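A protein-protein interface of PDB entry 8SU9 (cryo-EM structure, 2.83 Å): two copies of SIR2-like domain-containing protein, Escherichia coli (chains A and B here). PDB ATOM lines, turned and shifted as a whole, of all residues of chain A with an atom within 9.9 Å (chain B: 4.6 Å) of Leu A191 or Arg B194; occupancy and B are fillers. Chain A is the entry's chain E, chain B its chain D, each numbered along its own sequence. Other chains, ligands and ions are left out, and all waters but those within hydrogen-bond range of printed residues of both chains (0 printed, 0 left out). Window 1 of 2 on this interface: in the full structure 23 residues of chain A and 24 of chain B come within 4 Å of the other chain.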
ATOM      1  N   GLU A 132      17.625  14.767  -3.003  1.00  0.00           N
ATOM      2  CA  GLU A 132      17.718  14.321  -4.387  1.00  0.00           C
ATOM      3  C   GLU A 132      17.355  12.841  -4.484  1.00  0.00           C
ATOM      4  O   GLU A 132      16.849  12.233  -3.538  1.00  0.00           O
ATOM      5  CB  GLU A 132      19.113  14.601  -4.939  1.00  0.00           C
ATOM      6  CG  GLU A 132      19.639  15.990  -4.634  1.00  0.00           C
ATOM      7  CD  GLU A 132      18.907  17.078  -5.395  1.00  0.00           C
ATOM      8  OE1 GLU A 132      18.223  16.758  -6.390  1.00  0.00           O
ATOM      9  OE2 GLU A 132      19.016  18.256  -4.998  1.00  0.00           O
ATOM     10  N   LYS A 133      17.614  12.244  -5.643  1.00  0.00           N
ATOM     11  CA  LYS A 133      17.289  10.853  -5.904  1.00  0.00           C
ATOM     12  C   LYS A 133      18.524  10.111  -6.393  1.00  0.00           C
ATOM     13  O   LYS A 133      19.487  10.714  -6.876  1.00  0.00           O
ATOM     14  CB  LYS A 133      16.164  10.730  -6.937  1.00  0.00           C
ATOM     15  CG  LYS A 133      14.796  11.111  -6.407  1.00  0.00           C
ATOM     16  CD  LYS A 133      13.781  11.231  -7.532  1.00  0.00           C
ATOM     17  CE  LYS A 133      12.382  11.466  -6.990  1.00  0.00           C
ATOM     18  NZ  LYS A 133      12.391  12.364  -5.803  1.00  0.00           N
ATOM     19  N   ASN A 134      18.483   8.786  -6.253  1.00  0.00           N
ATOM     20  CA  ASN A 134      19.570   7.897  -6.663  1.00  0.00           C
ATOM     21  C   ASN A 134      20.868   8.243  -5.931  1.00  0.00           C
ATOM     22  O   ASN A 134      21.918   8.470  -6.535  1.00  0.00           O
ATOM     23  CB  ASN A 134      19.767   7.935  -8.182  1.00  0.00           C
ATOM     24  CG  ASN A 134      18.625   7.292  -8.934  1.00  0.00           C
ATOM     25  OD1 ASN A 134      18.512   6.070  -8.990  1.00  0.00           O
ATOM     26  ND2 ASN A 134      17.766   8.117  -9.519  1.00  0.00           N
ATOM     27  N   GLU A 178      18.014   0.005  -2.040  1.00  0.00           N
ATOM     28  CA  GLU A 178      17.162   0.395  -3.156  1.00  0.00           C
ATOM     29  C   GLU A 178      17.895   0.397  -4.490  1.00  0.00           C
ATOM     30  O   GLU A 178      17.242   0.492  -5.533  1.00  0.00           O
ATOM     31  CB  GLU A 178      16.555   1.773  -2.899  1.00  0.00           C
ATOM     32  CG  GLU A 178      15.237   1.728  -2.150  1.00  0.00           C
ATOM     33  CD  GLU A 178      14.806   3.086  -1.643  1.00  0.00           C
ATOM     34  OE1 GLU A 178      15.417   4.095  -2.051  1.00  0.00           O
ATOM     35  OE2 GLU A 178      13.860   3.146  -0.831  1.00  0.00           O
ATOM     36  N   ASP A 179      19.224   0.299  -4.486  1.00  0.00           N
ATOM     37  CA  ASP A 179      19.991   0.235  -5.722  1.00  0.00           C
ATOM     38  C   ASP A 179      20.144  -1.186  -6.243  1.00  0.00           C
ATOM     39  O   ASP A 179      20.131  -1.397  -7.461  1.00  0.00           O
ATOM     40  CB  ASP A 179      21.374   0.855  -5.516  1.00  0.00           C
ATOM     41  CG  ASP A 179      22.004   1.318  -6.811  1.00  0.00           C
ATOM     42  OD1 ASP A 179      21.601   2.385  -7.321  1.00  0.00           O
ATOM     43  OD2 ASP A 179      22.904   0.617  -7.321  1.00  0.00           O
ATOM     44  N   GLN A 183      14.180  -5.718  -1.204  1.00  0.00           N
ATOM     45  CA  GLN A 183      13.156  -5.094  -0.377  1.00  0.00           C
ATOM     46  C   GLN A 183      13.428  -5.411   1.085  1.00  0.00           C
ATOM     47  O   GLN A 183      13.649  -6.571   1.441  1.00  0.00           O
ATOM     48  CB  GLN A 183      11.761  -5.576  -0.776  1.00  0.00           C
ATOM     49  CG  GLN A 183      11.472  -5.458  -2.261  1.00  0.00           C
ATOM     50  CD  GLN A 183      10.010  -5.670  -2.589  1.00  0.00           C
ATOM     51  OE1 GLN A 183       9.157  -5.672  -1.702  1.00  0.00           O
ATOM     52  NE2 GLN A 183       9.712  -5.846  -3.870  1.00  0.00           N
ATOM     53  N   PHE A 188       6.646  -0.942   8.540  1.00  0.00           N
ATOM     54  CA  PHE A 188       5.730   0.071   8.040  1.00  0.00           C
ATOM     55  C   PHE A 188       5.082  -0.392   6.741  1.00  0.00           C
ATOM     56  O   PHE A 188       5.647  -1.188   5.987  1.00  0.00           O
ATOM     57  CB  PHE A 188       6.456   1.402   7.822  1.00  0.00           C
ATOM     58  CG  PHE A 188       6.745   2.152   9.091  1.00  0.00           C
ATOM     59  CD1 PHE A 188       7.716   1.709   9.970  1.00  0.00           C
ATOM     60  CD2 PHE A 188       6.041   3.296   9.409  1.00  0.00           C
ATOM     61  CE1 PHE A 188       7.980   2.395  11.137  1.00  0.00           C
ATOM     62  CE2 PHE A 188       6.300   3.985  10.576  1.00  0.00           C
ATOM     63  CZ  PHE A 188       7.272   3.534  11.439  1.00  0.00           C
ATOM     64  N   SER A 189       3.877   0.119   6.485  1.00  0.00           N
ATOM     65  CA  SER A 189       3.132  -0.237   5.284  1.00  0.00           C
ATOM     66  C   SER A 189       2.282   0.945   4.835  1.00  0.00           C
ATOM     67  O   SER A 189       1.655   1.612   5.661  1.00  0.00           O
ATOM     68  CB  SER A 189       2.245  -1.461   5.525  1.00  0.00           C
ATOM     69  OG  SER A 189       3.025  -2.628   5.708  1.00  0.00           O
ATOM     70  N   GLY A 190       2.261   1.190   3.532  1.00  0.00           N
ATOM     71  CA  GLY A 190       1.483   2.262   2.945  1.00  0.00           C
ATOM     72  C   GLY A 190       2.332   3.182   2.084  1.00  0.00           C
ATOM     73  O   GLY A 190       3.558   3.099   2.045  1.00  0.00           O
ATOM     74  N   LEU A 191       1.634   4.055   1.357  1.00  0.00           N
ATOM     75  CA  LEU A 191       2.313   5.086   0.580  1.00  0.00           C
ATOM     76  C   LEU A 191       1.799   6.482   0.911  1.00  0.00           C
ATOM     77  O   LEU A 191       2.589   7.420   1.051  1.00  0.00           O
ATOM     78  CB  LEU A 191       2.163   4.820  -0.920  1.00  0.00           C
ATOM     79  CG  LEU A 191       2.776   5.877  -1.842  1.00  0.00           C
ATOM     80  CD1 LEU A 191       4.240   6.101  -1.518  1.00  0.00           C
ATOM     81  CD2 LEU A 191       2.605   5.487  -3.298  1.00  0.00           C
ATOM     82  N   HIS A 192       0.484   6.633   1.043  1.00  0.00           N
ATOM     83  CA  HIS A 192      -0.104   7.935   1.323  1.00  0.00           C
ATOM     84  C   HIS A 192      -0.294   8.192   2.811  1.00  0.00           C
ATOM     85  O   HIS A 192      -0.271   9.353   3.232  1.00  0.00           O
ATOM     86  CB  HIS A 192      -1.442   8.075   0.591  1.00  0.00           C
ATOM     87  CG  HIS A 192      -1.332   7.909  -0.893  1.00  0.00           C
ATOM     88  ND1 HIS A 192      -0.623   8.783  -1.688  1.00  0.00           N
ATOM     89  CD2 HIS A 192      -1.832   6.967  -1.725  1.00  0.00           C
ATOM     90  CE1 HIS A 192      -0.695   8.388  -2.946  1.00  0.00           C
ATOM     91  NE2 HIS A 192      -1.421   7.287  -2.996  1.00  0.00           N
ATOM     92  N   THR A 193      -0.487   7.143   3.608  1.00  0.00           N
ATOM     93  CA  THR A 193      -0.431   7.232   5.066  1.00  0.00           C
ATOM     94  C   THR A 193       0.382   6.045   5.563  1.00  0.00           C
ATOM     95  O   THR A 193      -0.130   4.923   5.623  1.00  0.00           O
ATOM     96  CB  THR A 193      -1.823   7.235   5.696  1.00  0.00           C
ATOM     97  OG1 THR A 193      -2.569   6.107   5.224  1.00  0.00           O
ATOM     98  CG2 THR A 193      -2.566   8.513   5.354  1.00  0.00           C
ATOM     99  N   ARG A 194       1.640   6.290   5.912  1.00  0.00           N
ATOM    100  CA  ARG A 194       2.528   5.247   6.403  1.00  0.00           C
ATOM    101  C   ARG A 194       2.298   5.057   7.897  1.00  0.00           C
ATOM    102  O   ARG A 194       2.255   6.032   8.651  1.00  0.00           O
ATOM    103  CB  ARG A 194       3.985   5.617   6.127  1.00  0.00           C
ATOM    104  CG  ARG A 194       4.934   4.444   6.097  1.00  0.00           C
ATOM    105  CD  ARG A 194       4.856   3.750   4.758  1.00  0.00           C
ATOM    106  NE  ARG A 194       5.704   2.568   4.692  1.00  0.00           N
ATOM    107  CZ  ARG A 194       6.916   2.547   4.159  1.00  0.00           C
ATOM    108  NH1 ARG A 194       7.449   3.626   3.617  1.00  0.00           N
ATOM    109  NH2 ARG A 194       7.607   1.412   4.165  1.00  0.00           N
ATOM    110  N   GLN A 195       2.140   3.806   8.320  1.00  0.00           N
ATOM    111  CA  GLN A 195       1.826   3.489   9.704  1.00  0.00           C
ATOM    112  C   GLN A 195       2.684   2.325  10.178  1.00  0.00           C
ATOM    113  O   GLN A 195       3.228   1.560   9.378  1.00  0.00           O
ATOM    114  CB  GLN A 195       0.342   3.150   9.879  1.00  0.00           C
ATOM    115  CG  GLN A 195      -0.578   4.351   9.817  1.00  0.00           C
ATOM    116  CD  GLN A 195      -1.960   4.048  10.344  1.00  0.00           C
ATOM    117  OE1 GLN A 195      -2.160   3.076  11.070  1.00  0.00           O
ATOM    118  NE2 GLN A 195      -2.928   4.877   9.977  1.00  0.00           N
ATOM    119  N   TYR A 197       3.066  -1.190  12.023  1.00  0.00           N
ATOM    120  CA  TYR A 197       2.378  -2.427  12.392  1.00  0.00           C
ATOM    121  C   TYR A 197       3.389  -3.411  12.962  1.00  0.00           C
ATOM    122  O   TYR A 197       4.309  -3.833  12.236  1.00  0.00           O
ATOM    123  CB  TYR A 197       1.666  -3.038  11.187  1.00  0.00           C
ATOM    124  CG  TYR A 197       0.530  -2.206  10.642  1.00  0.00           C
ATOM    125  CD1 TYR A 197      -0.645  -2.047  11.361  1.00  0.00           C
ATOM    126  CD2 TYR A 197       0.628  -1.587   9.405  1.00  0.00           C
ATOM    127  CE1 TYR A 197      -1.687  -1.291  10.866  1.00  0.00           C
ATOM    128  CE2 TYR A 197      -0.409  -0.830   8.903  1.00  0.00           C
ATOM    129  CZ  TYR A 197      -1.564  -0.687   9.638  1.00  0.00           C
ATOM    130  OH  TYR A 197      -2.600   0.067   9.142  1.00  0.00           O
ATOM    131  N   TYR A 233       8.110  10.598  12.789  1.00  0.00           N
ATOM    132  CA  TYR A 233       7.554  11.671  13.603  1.00  0.00           C
ATOM    133  C   TYR A 233       6.124  11.321  13.988  1.00  0.00           C
ATOM    134  O   TYR A 233       5.488  10.464  13.372  1.00  0.00           O
ATOM    135  CB  TYR A 233       7.603  13.017  12.874  1.00  0.00           C
ATOM    136  CG  TYR A 233       6.647  13.132  11.710  1.00  0.00           C
ATOM    137  CD1 TYR A 233       6.912  12.500  10.505  1.00  0.00           C
ATOM    138  CD2 TYR A 233       5.485  13.880  11.815  1.00  0.00           C
ATOM    139  CE1 TYR A 233       6.042  12.605   9.439  1.00  0.00           C
ATOM    140  CE2 TYR A 233       4.610  13.991  10.754  1.00  0.00           C
ATOM    141  CZ  TYR A 233       4.894  13.351   9.571  1.00  0.00           C
ATOM    142  OH  TYR A 233       4.024  13.460   8.512  1.00  0.00           O
ATOM    143  N   ASN A 241       3.985   8.016  11.893  1.00  0.00           N
ATOM    144  CA  ASN A 241       4.022   8.012  10.439  1.00  0.00           C
ATOM    145  C   ASN A 241       5.457   8.084   9.933  1.00  0.00           C
ATOM    146  O   ASN A 241       6.369   8.519  10.639  1.00  0.00           O
ATOM    147  CB  ASN A 241       3.214   9.182   9.869  1.00  0.00           C
ATOM    148  CG  ASN A 241       1.745   9.100  10.215  1.00  0.00           C
ATOM    149  OD1 ASN A 241       1.212   9.963  10.910  1.00  0.00           O
ATOM    150  ND2 ASN A 241       1.079   8.059   9.731  1.00  0.00           N
ATOM    151  N   GLU A 242       5.643   7.649   8.689  1.00  0.00           N
ATOM    152  CA  GLU A 242       6.929   7.709   8.008  1.00  0.00           C
ATOM    153  C   GLU A 242       6.762   8.407   6.665  1.00  0.00           C
ATOM    154  O   GLU A 242       5.750   8.223   5.982  1.00  0.00           O
ATOM    155  CB  GLU A 242       7.517   6.312   7.799  1.00  0.00           C
ATOM    156  CG  GLU A 242       8.918   6.313   7.217  1.00  0.00           C
ATOM    157  CD  GLU A 242       9.390   4.929   6.831  1.00  0.00           C
ATOM    158  OE1 GLU A 242       8.545   4.099   6.439  1.00  0.00           O
ATOM    159  OE2 GLU A 242      10.606   4.667   6.923  1.00  0.00           O
ATOM    160  N   VAL A 243       7.756   9.209   6.292  1.00  0.00           N
ATOM    161  CA  VAL A 243       7.724   9.946   5.034  1.00  0.00           C
ATOM    162  C   VAL A 243       9.037   9.736   4.295  1.00  0.00           C
ATOM    163  O   VAL A 243       9.905   8.983   4.749  1.00  0.00           O
ATOM    164  CB  VAL A 243       7.457  11.444   5.265  1.00  0.00           C
ATOM    165  CG1 VAL A 243       6.052  11.663   5.787  1.00  0.00           C
ATOM    166  CG2 VAL A 243       8.480  12.021   6.223  1.00  0.00           C
ATOM    167  N   SER A 244       9.188  10.393   3.151  1.00  0.00           N
ATOM    168  CA  SER A 244      10.403  10.307   2.359  1.00  0.00           C
ATOM    169  C   SER A 244      11.400  11.383   2.783  1.00  0.00           C
ATOM    170  O   SER A 244      11.114  12.240   3.621  1.00  0.00           O
ATOM    171  CB  SER A 244      10.078  10.431   0.872  1.00  0.00           C
ATOM    172  OG  SER A 244      11.260  10.540   0.102  1.00  0.00           O
ATOM    173  N   GLN A 247      10.258  15.029   1.524  1.00  0.00           N
ATOM    174  CA  GLN A 247       9.154  15.569   2.307  1.00  0.00           C
ATOM    175  C   GLN A 247       9.614  15.976   3.701  1.00  0.00           C
ATOM    176  O   GLN A 247       9.228  17.036   4.203  1.00  0.00           O
ATOM    177  CB  GLN A 247       8.019  14.549   2.377  1.00  0.00           C
ATOM    178  CG  GLN A 247       6.674  15.136   2.765  1.00  0.00           C
ATOM    179  CD  GLN A 247       5.529  14.184   2.498  1.00  0.00           C
ATOM    180  OE1 GLN A 247       5.704  13.150   1.856  1.00  0.00           O
ATOM    181  NE2 GLN A 247       4.347  14.525   2.996  1.00  0.00           N
ATOM    182  N   GLU B 178      -6.221   1.733   2.234  1.00  0.00           N
ATOM    183  CA  GLU B 178      -5.311   2.090   3.315  1.00  0.00           C
ATOM    184  C   GLU B 178      -6.029   2.284   4.644  1.00  0.00           C
ATOM    185  O   GLU B 178      -5.377   2.265   5.692  1.00  0.00           O
ATOM    186  CB  GLU B 178      -4.532   3.354   2.956  1.00  0.00           C
ATOM    187  CG  GLU B 178      -3.183   3.079   2.314  1.00  0.00           C
ATOM    188  CD  GLU B 178      -2.587   4.303   1.652  1.00  0.00           C
ATOM    189  OE1 GLU B 178      -3.042   5.425   1.954  1.00  0.00           O
ATOM    190  OE2 GLU B 178      -1.668   4.145   0.823  1.00  0.00           O
ATOM    191  N   PHE B 188       4.924  -1.296  -8.384  1.00  0.00           N
ATOM    192  CA  PHE B 188       5.992  -0.407  -7.960  1.00  0.00           C
ATOM    193  C   PHE B 188       6.608  -0.895  -6.651  1.00  0.00           C
ATOM    194  O   PHE B 188       5.957  -1.558  -5.842  1.00  0.00           O
ATOM    195  CB  PHE B 188       5.470   1.023  -7.797  1.00  0.00           C
ATOM    196  CG  PHE B 188       5.119   1.700  -9.092  1.00  0.00           C
ATOM    197  CD1 PHE B 188       4.015   1.301  -9.823  1.00  0.00           C
ATOM    198  CD2 PHE B 188       5.887   2.742  -9.574  1.00  0.00           C
ATOM    199  CE1 PHE B 188       3.691   1.924 -11.008  1.00  0.00           C
ATOM    200  CE2 PHE B 188       5.567   3.366 -10.760  1.00  0.00           C
ATOM    201  CZ  PHE B 188       4.468   2.957 -11.476  1.00  0.00           C
ATOM    202  N   SER B 189       7.883  -0.557  -6.452  1.00  0.00           N
ATOM    203  CA  SER B 189       8.598  -0.952  -5.245  1.00  0.00           C
ATOM    204  C   SER B 189       9.559   0.152  -4.828  1.00  0.00           C
ATOM    205  O   SER B 189      10.091   0.881  -5.668  1.00  0.00           O
ATOM    206  CB  SER B 189       9.366  -2.262  -5.448  1.00  0.00           C
ATOM    207  OG  SER B 189      10.056  -2.632  -4.269  1.00  0.00           O
ATOM    208  N   GLY B 190       9.780   0.264  -3.526  1.00  0.00           N
ATOM    209  CA  GLY B 190      10.671   1.256  -2.960  1.00  0.00           C
ATOM    210  C   GLY B 190       9.916   2.402  -2.304  1.00  0.00           C
ATOM    211  O   GLY B 190       8.720   2.607  -2.508  1.00  0.00           O
ATOM    212  N   LEU B 191      10.653   3.153  -1.483  1.00  0.00           N
ATOM    213  CA  LEU B 191      10.116   4.335  -0.815  1.00  0.00           C
ATOM    214  C   LEU B 191      10.822   5.617  -1.236  1.00  0.00           C
ATOM    215  O   LEU B 191      10.165   6.548  -1.706  1.00  0.00           O
ATOM    216  CB  LEU B 191      10.193   4.169   0.706  1.00  0.00           C
ATOM    217  CG  LEU B 191       9.873   5.442   1.492  1.00  0.00           C
ATOM    218  CD1 LEU B 191       8.424   5.846   1.300  1.00  0.00           C
ATOM    219  CD2 LEU B 191      10.198   5.269   2.965  1.00  0.00           C
ATOM    220  N   HIS B 192      12.144   5.698  -1.074  1.00  0.00           N
ATOM    221  CA  HIS B 192      12.860   6.917  -1.436  1.00  0.00           C
ATOM    222  C   HIS B 192      12.996   7.064  -2.944  1.00  0.00           C
ATOM    223  O   HIS B 192      12.999   8.187  -3.456  1.00  0.00           O
ATOM    224  CB  HIS B 192      14.237   6.935  -0.772  1.00  0.00           C
ATOM    225  CG  HIS B 192      14.182   6.865   0.722  1.00  0.00           C
ATOM    226  ND1 HIS B 192      13.807   7.935   1.504  1.00  0.00           N
ATOM    227  CD2 HIS B 192      14.449   5.850   1.578  1.00  0.00           C
ATOM    228  CE1 HIS B 192      13.845   7.583   2.776  1.00  0.00           C
ATOM    229  NE2 HIS B 192      14.234   6.324   2.848  1.00  0.00           N
ATOM    230  N   THR B 193      13.107   5.951  -3.663  1.00  0.00           N
ATOM    231  CA  THR B 193      13.086   5.940  -5.121  1.00  0.00           C
ATOM    232  C   THR B 193      12.140   4.833  -5.563  1.00  0.00           C
ATOM    233  O   THR B 193      12.529   3.663  -5.615  1.00  0.00           O
ATOM    234  CB  THR B 193      14.483   5.729  -5.701  1.00  0.00           C
ATOM    235  OG1 THR B 193      15.425   6.531  -4.979  1.00  0.00           O
ATOM    236  CG2 THR B 193      14.514   6.119  -7.166  1.00  0.00           C
ATOM    237  N   ARG B 194      10.902   5.203  -5.878  1.00  0.00           N
ATOM    238  CA  ARG B 194       9.871   4.260  -6.296  1.00  0.00           C
ATOM    239  C   ARG B 194       9.982   4.061  -7.805  1.00  0.00           C
ATOM    240  O   ARG B 194       9.956   5.032  -8.567  1.00  0.00           O
ATOM    241  CB  ARG B 194       8.487   4.771  -5.901  1.00  0.00           C
ATOM    242  CG  ARG B 194       7.357   3.837  -6.275  1.00  0.00           C
ATOM    243  CD  ARG B 194       7.365   2.603  -5.404  1.00  0.00           C
ATOM    244  NE  ARG B 194       6.955   2.872  -4.032  1.00  0.00           N
ATOM    245  CZ  ARG B 194       5.701   2.836  -3.605  1.00  0.00           C
ATOM    246  NH1 ARG B 194       4.705   2.519  -4.415  1.00  0.00           N
ATOM    247  NH2 ARG B 194       5.441   3.108  -2.331  1.00  0.00           N
ATOM    248  N   GLN B 195      10.113   2.807  -8.233  1.00  0.00           N
ATOM    249  CA  GLN B 195      10.279   2.462  -9.637  1.00  0.00           C
ATOM    250  C   GLN B 195       9.295   1.368 -10.031  1.00  0.00           C
ATOM    251  O   GLN B 195       8.647   0.754  -9.183  1.00  0.00           O
ATOM    252  CB  GLN B 195      11.710   2.002  -9.931  1.00  0.00           C
ATOM    253  CG  GLN B 195      12.659   3.127 -10.288  1.00  0.00           C
ATOM    254  CD  GLN B 195      13.998   2.620 -10.770  1.00  0.00           C
ATOM    255  OE1 GLN B 195      14.090   1.547 -11.361  1.00  0.00           O
ATOM    256  NE2 GLN B 195      15.048   3.391 -10.517  1.00  0.00           N
ATOM    257  N   VAL B 240       9.929   4.968 -14.862  1.00  0.00           N
ATOM    258  CA  VAL B 240       8.706   5.564 -14.341  1.00  0.00           C
ATOM    259  C   VAL B 240       8.794   5.577 -12.823  1.00  0.00           C
ATOM    260  O   VAL B 240       9.104   4.552 -12.207  1.00  0.00           O
ATOM    261  CB  VAL B 240       7.456   4.800 -14.811  1.00  0.00           C
ATOM    262  CG1 VAL B 240       6.205   5.601 -14.519  1.00  0.00           C
ATOM    263  CG2 VAL B 240       7.553   4.493 -16.291  1.00  0.00           C
ATOM    264  N   ASN B 241       8.528   6.734 -12.224  1.00  0.00           N
ATOM    265  CA  ASN B 241       8.604   6.915 -10.781  1.00  0.00           C
ATOM    266  C   ASN B 241       7.247   7.322 -10.224  1.00  0.00           C
ATOM    267  O   ASN B 241       6.528   8.118 -10.834  1.00  0.00           O
ATOM    268  CB  ASN B 241       9.652   7.968 -10.415  1.00  0.00           C
ATOM    269  CG  ASN B 241      11.065   7.514 -10.714  1.00  0.00           C
ATOM    270  OD1 ASN B 241      11.657   7.909 -11.716  1.00  0.00           O
ATOM    271  ND2 ASN B 241      11.616   6.685  -9.838  1.00  0.00           N
ATOM    272  N   GLU B 242       6.904   6.771  -9.063  1.00  0.00           N
ATOM    273  CA  GLU B 242       5.672   7.094  -8.360  1.00  0.00           C
ATOM    274  C   GLU B 242       5.978   7.890  -7.098  1.00  0.00           C
ATOM    275  O   GLU B 242       6.976   7.654  -6.413  1.00  0.00           O
ATOM    276  CB  GLU B 242       4.892   5.826  -7.998  1.00  0.00           C
ATOM    277  CG  GLU B 242       3.518   6.090  -7.405  1.00  0.00           C
ATOM    278  CD  GLU B 242       2.773   4.817  -7.069  1.00  0.00           C
ATOM    279  OE1 GLU B 242       3.353   3.725  -7.238  1.00  0.00           O
ATOM    280  OE2 GLU B 242       1.607   4.909  -6.632  1.00  0.00           O
ATOM    281  N   SER B 244       3.998  10.225  -3.667  1.00  0.00           N
ATOM    282  CA  SER B 244       2.804  10.326  -2.840  1.00  0.00           C
ATOM    283  C   SER B 244       1.944  11.517  -3.269  1.00  0.00           C
ATOM    284  O   SER B 244       2.289  12.282  -4.175  1.00  0.00           O
ATOM    285  CB  SER B 244       3.188  10.437  -1.367  1.00  0.00           C
ATOM    286  OG  SER B 244       3.610  11.748  -1.045  1.00  0.00           O
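The side-chain carboxylate (OE2) of Glu B178 sits at hydrogen-bond distance from the backbone NH (N) of Leu A191, 3.3 Å away.
N of His A192 sits at hydrogen-bond distance from OE2 of Glu B178 (3.3 Å).
OE1 of Glu B178 is in hydrogen-bond range of OG1 of Thr A193, 3.4 Å away.
The side-chain hydroxyl (OG) of Ser B189 lies within hydrogen-bond range of the side-chain amide nitrogen (NE2) of Gln A183, 3.3 Å away.
N of Leu B191 lies within hydrogen-bond range of OE2 of Glu A178 (3.3 Å).
The backbone NH of His B192 lies within hydrogen-bond range of the side-chain carboxylate of Glu A178, at 3.1 Å.
N of Thr B193 is in hydrogen-bond range of OE1 of Glu A178 (3.4 Å).
The backbone NH (N) of Ser B189 sits at hydrogen-bond distance from the backbone carbonyl oxygen (O) of Gln B195 (3.1 Å).
The backbone carbonyl oxygen (O) of Gly B190 lies close to the guanidinium group (NH2) of Arg B194 (3.3 Å).
O of Arg B194 is in hydrogen-bond range of ND2 of Asn B241 (2.7 Å).
NH1 of Arg B194 is in salt-bridge range of OE1 of Glu B242 (3.4 Å).
The backbone carbonyl oxygen (O) of Gly A190 sits close to the guanidinium group (NE) of Arg A194 (3.4 Å).
The side-chain amide nitrogen (ND2) of Asn A241 sits at hydrogen-bond distance from the backbone carbonyl oxygen (O) of Arg A194, at 2.6 Å.
Leu A191 touches Arg B194.
CD2 of Leu A191 touches OE2 of Glu B242 (3.5 Å).
Leu A191 touches Ser B244 (O to CB, 3.9 Å).
CA of Ser B244 touches ND1 of His A192 (3.9 Å).
Leu B191 touches Arg A194 (CD2 to NH1, 3.3 Å).
CD2 of Leu B191 touches CD of Glu A242 (3.96 Å).
Ser A244 touches His B192.
OG of Ser B244 touches OE1 of Gln A247 (3.8 Å).
Of chain B, only Glu B178, Arg B194, Glu B242 and Ser B244 come within 4 Å of Leu A191.
Of the printed residues of chain A, Arg B194 touches Leu A191 (3.3 Å).
Gly B190 touches none of the printed residues of chain A.
Of the printed residues of chain A, Glu B242 touches Leu A191.
Printed residues of chain B within 4 Å of His A192: Glu B178 and Ser B244.
Printed residues of chain B within 4 Å of Gln A247: Ser B244 (3.8 Å).
Of the printed residues of chain A, His B192 touches Glu A178 (3.1 Å) and Ser A244 (3.9 Å).
The nearest printed residue of chain B that does not touch Leu A191 is Leu B191 (5.1 Å).
The nearest residue of chain A that does not touch Arg B194 is Gly A190 (4.8 Å).
Of the 13 printed residues of chain B, 8 touch a printed residue of chain A.
Hydrophobic or aromatic side chains of chain B within 4 Å of the printed part of chain A: Leu B191 and His B192.
Printed residues of chain A that touch a printed residue of chain B: Glu A178, Gln A183, Leu A191, His A192, Thr A193, Arg A194, Glu A242, Ser A244 and Gln A247.
Hydrophobic or aromatic side chains of chain A that line the printed part of chain B: Leu A191 and His A192.
Among the printed residues, no Asp or Glu carboxylate lies within 4 Å of a Lys or Arg side-chain nitrogen of the other chain.
Glu A178 touches Leu B191, and with the chains exchanged Leu A191 touches Glu B178.
Glu A178 touches Thr B193, and with the chains exchanged Thr A193 touches Glu B178.
Leu A191 touches Arg B194, and with the chains exchanged Arg A194 touches Leu B191.
Leu A191 touches Glu B242, and with the chains exchanged Glu A242 touches Leu B191.
Positions printed for both chains: 178, 188, 189, 190, 191, 192, 193, 194, 195, 241, 242 and 244.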
